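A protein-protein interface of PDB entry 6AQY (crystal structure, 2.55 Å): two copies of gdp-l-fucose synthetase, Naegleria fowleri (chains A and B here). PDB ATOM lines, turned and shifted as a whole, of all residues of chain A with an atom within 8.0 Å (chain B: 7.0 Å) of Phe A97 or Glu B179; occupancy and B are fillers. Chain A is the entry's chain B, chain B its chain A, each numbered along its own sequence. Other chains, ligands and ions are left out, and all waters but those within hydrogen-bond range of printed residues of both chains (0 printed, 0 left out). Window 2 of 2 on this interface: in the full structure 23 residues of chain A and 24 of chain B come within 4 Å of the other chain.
The side-chain carboxylate of Glu B174 lies within salt-bridge range of the side-chain amino group of Lys A98 (3.8 Å).
OH of Tyr B117 sits at hydrogen-bond distance from OE1 of Glu B179, 2.6 Å away.
The side-chain amide nitrogen of Asn B178 lies within hydrogen-bond range of the backbone carbonyl oxygen of Glu B174 (3.3 Å).
Among the printed residues, pairs that only touch across the chains: Ala A157 with Trp B171, Lys A98 with Trp B171, Trp A102 with Trp B171, Phe A97 with Asn B178, Val A99 with Trp B171, Phe A97 with Glu B179 and Phe A97 with Lys B175.
Phe A97 touches just these residues of chain B: Lys B175, Asn B178 and Glu B179.
Printed residues of chain B within 4 Å of Lys A98: Trp B171 and Glu B174.
Of the printed residues of chain B, Trp A102 touches Trp B171 (3.5 Å).
Printed residues of chain B within 4 Å of Ala A157: Trp B171 (3.4 Å).
Of the printed residues of chain A, Trp B171 touches Lys A98 (3.5 Å), Val A99 (3.6 Å), Trp A102 (3.5 Å) and Ala A157 (3.4 Å).
No residue of chain A comes within 4 Å of Gly B180.
Ser B182 touches none of the printed residues of chain A.
The nearest residue of chain B that does not touch Phe A97 is Glu B174 (5.4 Å).
Of the 9 printed residues of chain A, 5 touch a printed residue of chain B.
Hydrophobic or aromatic side chains of chain A that line the printed part of chain B: Phe A97, Val A99, Trp A102 and Ala A157.
Of the 11 printed residues of chain B, 5 touch a printed residue of chain A.
Printed residues of chain B that touch a printed residue of chain A: Trp B171, Glu B174, Lys B175, Asn B178 and Glu B179.
Hydrophobic or aromatic side chains of chain B within 4 Å of the printed part of chain A: Trp B171.
Among the printed residues, Asp or Glu carboxylates within 4 Å of a Lys or Arg side-chain nitrogen of the other chain: Lys A98 with Glu B174.
No position is printed for both chains.
Of the 8 pairs that touch across the chains among the printed residues, none has its exchanged pair printed and touching as well.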
ATOM      1  N   PHE A  97     -16.457 -29.821  30.239  1.00  0.00           N
ATOM      2  CA  PHE A  97     -16.990 -29.445  28.920  1.00  0.00           C
ATOM      3  C   PHE A  97     -16.983 -27.932  28.734  1.00  0.00           C
ATOM      4  O   PHE A  97     -17.293 -27.200  29.666  1.00  0.00           O
ATOM      5  CB  PHE A  97     -18.432 -29.943  28.743  1.00  0.00           C
ATOM      6  CG  PHE A  97     -18.547 -31.416  28.491  1.00  0.00           C
ATOM      7  CD1 PHE A  97     -17.901 -32.008  27.420  1.00  0.00           C
ATOM      8  CD2 PHE A  97     -19.294 -32.215  29.348  1.00  0.00           C
ATOM      9  CE1 PHE A  97     -18.012 -33.365  27.199  1.00  0.00           C
ATOM     10  CE2 PHE A  97     -19.404 -33.557  29.146  1.00  0.00           C
ATOM     11  CZ  PHE A  97     -18.767 -34.142  28.068  1.00  0.00           C
ATOM     12  N   LYS A  98     -16.694 -27.478  27.507  1.00  0.00           N
ATOM     13  CA  LYS A  98     -16.707 -26.047  27.208  1.00  0.00           C
ATOM     14  C   LYS A  98     -18.085 -25.450  27.454  1.00  0.00           C
ATOM     15  O   LYS A  98     -18.211 -24.296  27.897  1.00  0.00           O
ATOM     16  CB  LYS A  98     -16.285 -25.815  25.759  1.00  0.00           C
ATOM     17  CG  LYS A  98     -14.812 -25.606  25.544  1.00  0.00           C
ATOM     18  CD  LYS A  98     -14.586 -25.351  24.078  1.00  0.00           C
ATOM     19  CE  LYS A  98     -13.151 -25.030  23.726  1.00  0.00           C
ATOM     20  NZ  LYS A  98     -13.138 -24.720  22.266  1.00  0.00           N
ATOM     21  N   VAL A  99     -19.127 -26.235  27.182  1.00  0.00           N
ATOM     22  CA  VAL A  99     -20.492 -25.843  27.494  1.00  0.00           C
ATOM     23  C   VAL A  99     -20.602 -25.336  28.930  1.00  0.00           C
ATOM     24  O   VAL A  99     -21.170 -24.273  29.172  1.00  0.00           O
ATOM     25  CB  VAL A  99     -21.438 -27.023  27.226  1.00  0.00           C
ATOM     26  CG1 VAL A  99     -22.877 -26.738  27.709  1.00  0.00           C
ATOM     27  CG2 VAL A  99     -21.439 -27.286  25.759  1.00  0.00           C
ATOM     28  N   SER A 100     -20.052 -26.078  29.902  1.00  0.00           N
ATOM     29  CA  SER A 100     -20.176 -25.653  31.298  1.00  0.00           C
ATOM     30  C   SER A 100     -19.467 -24.332  31.544  1.00  0.00           C
ATOM     31  O   SER A 100     -19.991 -23.459  32.245  1.00  0.00           O
ATOM     32  CB  SER A 100     -19.610 -26.697  32.245  1.00  0.00           C
ATOM     33  OG  SER A 100     -20.260 -27.925  32.076  1.00  0.00           O
ATOM     34  N   PHE A 101     -18.267 -24.165  30.988  1.00  0.00           N
ATOM     35  CA  PHE A 101     -17.551 -22.918  31.225  1.00  0.00           C
ATOM     36  C   PHE A 101     -18.259 -21.740  30.606  1.00  0.00           C
ATOM     37  O   PHE A 101     -18.204 -20.643  31.168  1.00  0.00           O
ATOM     38  CB  PHE A 101     -16.113 -23.025  30.757  1.00  0.00           C
ATOM     39  CG  PHE A 101     -15.363 -24.065  31.495  1.00  0.00           C
ATOM     40  CD1 PHE A 101     -15.108 -23.900  32.849  1.00  0.00           C
ATOM     41  CD2 PHE A 101     -14.970 -25.246  30.870  1.00  0.00           C
ATOM     42  CE1 PHE A 101     -14.442 -24.869  33.560  1.00  0.00           C
ATOM     43  CE2 PHE A 101     -14.292 -26.217  31.578  1.00  0.00           C
ATOM     44  CZ  PHE A 101     -14.031 -26.037  32.924  1.00  0.00           C
ATOM     45  N   TRP A 102     -18.922 -21.925  29.462  1.00  0.00           N
ATOM     46  CA  TRP A 102     -19.698 -20.817  28.913  1.00  0.00           C
ATOM     47  C   TRP A 102     -20.872 -20.496  29.831  1.00  0.00           C
ATOM     48  O   TRP A 102     -21.027 -19.345  30.265  1.00  0.00           O
ATOM     49  CB  TRP A 102     -20.185 -21.096  27.484  1.00  0.00           C
ATOM     50  CG  TRP A 102     -21.270 -20.111  27.109  1.00  0.00           C
ATOM     51  CD1 TRP A 102     -22.612 -20.370  26.992  1.00  0.00           C
ATOM     52  CD2 TRP A 102     -21.120 -18.694  26.892  1.00  0.00           C
ATOM     53  NE1 TRP A 102     -23.291 -19.209  26.696  1.00  0.00           N
ATOM     54  CE2 TRP A 102     -22.399 -18.172  26.630  1.00  0.00           C
ATOM     55  CE3 TRP A 102     -20.022 -17.824  26.865  1.00  0.00           C
ATOM     56  CZ2 TRP A 102     -22.613 -16.818  26.343  1.00  0.00           C
ATOM     57  CZ3 TRP A 102     -20.232 -16.487  26.572  1.00  0.00           C
ATOM     58  CH2 TRP A 102     -21.516 -15.992  26.322  1.00  0.00           C
ATOM     59  N   LEU A 103     -21.667 -21.515  30.179  1.00  0.00           N
ATOM     60  CA  LEU A 103     -22.894 -21.322  30.953  1.00  0.00           C
ATOM     61  C   LEU A 103     -22.616 -20.868  32.387  1.00  0.00           C
ATOM     62  O   LEU A 103     -23.282 -19.961  32.893  1.00  0.00           O
ATOM     63  CB  LEU A 103     -23.741 -22.604  30.944  1.00  0.00           C
ATOM     64  CG  LEU A 103     -24.329 -23.021  29.580  1.00  0.00           C
ATOM     65  CD1 LEU A 103     -25.104 -24.329  29.669  1.00  0.00           C
ATOM     66  CD2 LEU A 103     -25.196 -21.959  28.963  1.00  0.00           C
ATOM     67  N   ASP A 104     -21.681 -21.516  33.078  1.00  0.00           N
ATOM     68  CA  ASP A 104     -21.459 -21.178  34.486  1.00  0.00           C
ATOM     69  C   ASP A 104     -20.943 -19.756  34.643  1.00  0.00           C
ATOM     70  O   ASP A 104     -21.421 -19.011  35.502  1.00  0.00           O
ATOM     71  CB  ASP A 104     -20.515 -22.185  35.137  1.00  0.00           C
ATOM     72  CG  ASP A 104     -21.172 -23.576  35.302  1.00  0.00           C
ATOM     73  OD1 ASP A 104     -22.414 -23.659  35.160  1.00  0.00           O
ATOM     74  OD2 ASP A 104     -20.466 -24.568  35.604  1.00  0.00           O
ATOM     75  N   ALA A 157     -14.490 -20.711  25.367  1.00  0.00           N
ATOM     76  CA  ALA A 157     -15.695 -20.511  26.177  1.00  0.00           C
ATOM     77  C   ALA A 157     -15.410 -19.599  27.370  1.00  0.00           C
ATOM     78  O   ALA A 157     -16.133 -18.627  27.607  1.00  0.00           O
ATOM     79  CB  ALA A 157     -16.261 -21.862  26.647  1.00  0.00           C
ATOM     80  N   TYR B 117     -30.074 -30.245  23.314  1.00  0.00           N
ATOM     81  CA  TYR B 117     -29.111 -31.281  23.660  1.00  0.00           C
ATOM     82  C   TYR B 117     -29.717 -32.282  24.633  1.00  0.00           C
ATOM     83  O   TYR B 117     -29.634 -33.497  24.421  1.00  0.00           O
ATOM     84  CB  TYR B 117     -27.838 -30.669  24.270  1.00  0.00           C
ATOM     85  CG  TYR B 117     -26.764 -31.719  24.423  1.00  0.00           C
ATOM     86  CD1 TYR B 117     -26.672 -32.483  25.573  1.00  0.00           C
ATOM     87  CD2 TYR B 117     -25.893 -32.013  23.366  1.00  0.00           C
ATOM     88  CE1 TYR B 117     -25.701 -33.469  25.697  1.00  0.00           C
ATOM     89  CE2 TYR B 117     -24.932 -32.994  23.476  1.00  0.00           C
ATOM     90  CZ  TYR B 117     -24.838 -33.721  24.643  1.00  0.00           C
ATOM     91  OH  TYR B 117     -23.888 -34.714  24.745  1.00  0.00           O
ATOM     92  N   TRP B 171     -20.051 -25.488  20.699  1.00  0.00           N
ATOM     93  CA  TRP B 171     -19.678 -26.148  21.951  1.00  0.00           C
ATOM     94  C   TRP B 171     -20.554 -27.364  22.199  1.00  0.00           C
ATOM     95  O   TRP B 171     -20.065 -28.415  22.624  1.00  0.00           O
ATOM     96  CB  TRP B 171     -19.763 -25.164  23.113  1.00  0.00           C
ATOM     97  CG  TRP B 171     -18.717 -24.120  22.975  1.00  0.00           C
ATOM     98  CD1 TRP B 171     -17.480 -24.294  22.456  1.00  0.00           C
ATOM     99  CD2 TRP B 171     -18.826 -22.719  23.297  1.00  0.00           C
ATOM    100  NE1 TRP B 171     -16.789 -23.108  22.464  1.00  0.00           N
ATOM    101  CE2 TRP B 171     -17.590 -22.124  22.979  1.00  0.00           C
ATOM    102  CE3 TRP B 171     -19.836 -21.922  23.845  1.00  0.00           C
ATOM    103  CZ2 TRP B 171     -17.336 -20.771  23.177  1.00  0.00           C
ATOM    104  CZ3 TRP B 171     -19.578 -20.574  24.052  1.00  0.00           C
ATOM    105  CH2 TRP B 171     -18.334 -20.017  23.717  1.00  0.00           C
ATOM    106  N   GLU B 174     -19.321 -30.081  20.043  1.00  0.00           N
ATOM    107  CA  GLU B 174     -18.182 -30.672  20.720  1.00  0.00           C
ATOM    108  C   GLU B 174     -18.644 -31.641  21.795  1.00  0.00           C
ATOM    109  O   GLU B 174     -18.149 -32.770  21.879  1.00  0.00           O
ATOM    110  CB  GLU B 174     -17.342 -29.557  21.329  1.00  0.00           C
ATOM    111  CG  GLU B 174     -15.871 -29.760  21.302  1.00  0.00           C
ATOM    112  CD  GLU B 174     -15.129 -28.486  21.646  1.00  0.00           C
ATOM    113  OE1 GLU B 174     -14.251 -28.543  22.541  1.00  0.00           O
ATOM    114  OE2 GLU B 174     -15.432 -27.435  21.035  1.00  0.00           O
ATOM    115  N   LYS B 175     -19.651 -31.250  22.581  1.00  0.00           N
ATOM    116  CA  LYS B 175     -20.113 -32.138  23.642  1.00  0.00           C
ATOM    117  C   LYS B 175     -20.746 -33.414  23.076  1.00  0.00           C
ATOM    118  O   LYS B 175     -20.497 -34.513  23.590  1.00  0.00           O
ATOM    119  CB  LYS B 175     -21.111 -31.420  24.541  1.00  0.00           C
ATOM    120  CG  LYS B 175     -21.524 -32.242  25.720  1.00  0.00           C
ATOM    121  CD  LYS B 175     -22.542 -31.533  26.556  1.00  0.00           C
ATOM    122  CE  LYS B 175     -22.914 -32.378  27.746  1.00  0.00           C
ATOM    123  NZ  LYS B 175     -23.625 -31.555  28.720  1.00  0.00           N
ATOM    124  N   ALA B 176     -21.574 -33.280  22.024  1.00  0.00           N
ATOM    125  CA  ALA B 176     -22.272 -34.430  21.450  1.00  0.00           C
ATOM    126  C   ALA B 176     -21.296 -35.509  21.010  1.00  0.00           C
ATOM    127  O   ALA B 176     -21.533 -36.698  21.240  1.00  0.00           O
ATOM    128  CB  ALA B 176     -23.141 -33.991  20.269  1.00  0.00           C
ATOM    129  N   VAL B 177     -20.190 -35.106  20.388  1.00  0.00           N
ATOM    130  CA  VAL B 177     -19.135 -36.047  20.017  1.00  0.00           C
ATOM    131  C   VAL B 177     -18.577 -36.755  21.246  1.00  0.00           C
ATOM    132  O   VAL B 177     -18.573 -37.989  21.321  1.00  0.00           O
ATOM    133  CB  VAL B 177     -18.021 -35.322  19.240  1.00  0.00           C
ATOM    134  CG1 VAL B 177     -16.888 -36.264  19.037  1.00  0.00           C
ATOM    135  CG2 VAL B 177     -18.542 -34.794  17.913  1.00  0.00           C
ATOM    136  N   ASN B 178     -18.125 -35.988  22.241  1.00  0.00           N
ATOM    137  CA  ASN B 178     -17.503 -36.604  23.409  1.00  0.00           C
ATOM    138  C   ASN B 178     -18.437 -37.579  24.100  1.00  0.00           C
ATOM    139  O   ASN B 178     -17.986 -38.600  24.618  1.00  0.00           O
ATOM    140  CB  ASN B 178     -17.062 -35.529  24.402  1.00  0.00           C
ATOM    141  CG  ASN B 178     -15.999 -34.613  23.835  1.00  0.00           C
ATOM    142  OD1 ASN B 178     -15.180 -35.022  23.016  1.00  0.00           O
ATOM    143  ND2 ASN B 178     -16.006 -33.364  24.274  1.00  0.00           N
ATOM    144  N   GLU B 179     -19.736 -37.331  24.057  1.00  0.00           N
ATOM    145  CA  GLU B 179     -20.692 -38.212  24.703  1.00  0.00           C
ATOM    146  C   GLU B 179     -21.306 -39.229  23.745  1.00  0.00           C
ATOM    147  O   GLU B 179     -22.148 -40.032  24.162  1.00  0.00           O
ATOM    148  CB  GLU B 179     -21.796 -37.388  25.364  1.00  0.00           C
ATOM    149  CG  GLU B 179     -21.349 -36.629  26.599  1.00  0.00           C
ATOM    150  CD  GLU B 179     -22.518 -36.179  27.490  1.00  0.00           C
ATOM    151  OE1 GLU B 179     -23.664 -35.998  26.997  1.00  0.00           O
ATOM    152  OE2 GLU B 179     -22.280 -36.021  28.704  1.00  0.00           O
ATOM    153  N   GLY B 180     -20.871 -39.247  22.491  1.00  0.00           N
ATOM    154  CA  GLY B 180     -21.428 -40.179  21.532  1.00  0.00           C
ATOM    155  C   GLY B 180     -22.894 -39.979  21.204  1.00  0.00           C
ATOM    156  O   GLY B 180     -23.566 -40.941  20.815  1.00  0.00           O
ATOM    157  N   LYS B 181     -23.398 -38.748  21.299  1.00  0.00           N
ATOM    158  CA  LYS B 181     -24.781 -38.424  20.959  1.00  0.00           C
ATOM    159  C   LYS B 181     -24.905 -37.917  19.526  1.00  0.00           C
ATOM    160  O   LYS B 181     -24.022 -37.223  19.004  1.00  0.00           O
ATOM    161  CB  LYS B 181     -25.340 -37.350  21.895  1.00  0.00           C
ATOM    162  CG  LYS B 181     -25.942 -37.863  23.162  1.00  0.00           C
ATOM    163  CD  LYS B 181     -26.395 -36.704  24.002  1.00  0.00           C
ATOM    164  CE  LYS B 181     -27.860 -36.416  23.822  1.00  0.00           C
ATOM    165  NZ  LYS B 181     -28.489 -36.360  25.166  1.00  0.00           N
ATOM    166  N   SER B 182     -26.050 -38.226  18.916  1.00  0.00           N
ATOM    167  CA  SER B 182     -26.390 -37.777  17.563  1.00  0.00           C
ATOM    168  C   SER B 182     -27.165 -36.464  17.674  1.00  0.00           C
ATOM    169  O   SER B 182     -28.395 -36.417  17.617  1.00  0.00           O
ATOM    170  CB  SER B 182     -27.222 -38.823  16.838  1.00  0.00           C
ATOM    171  OG  SER B 182     -26.497 -39.990  16.550  1.00  0.00           O
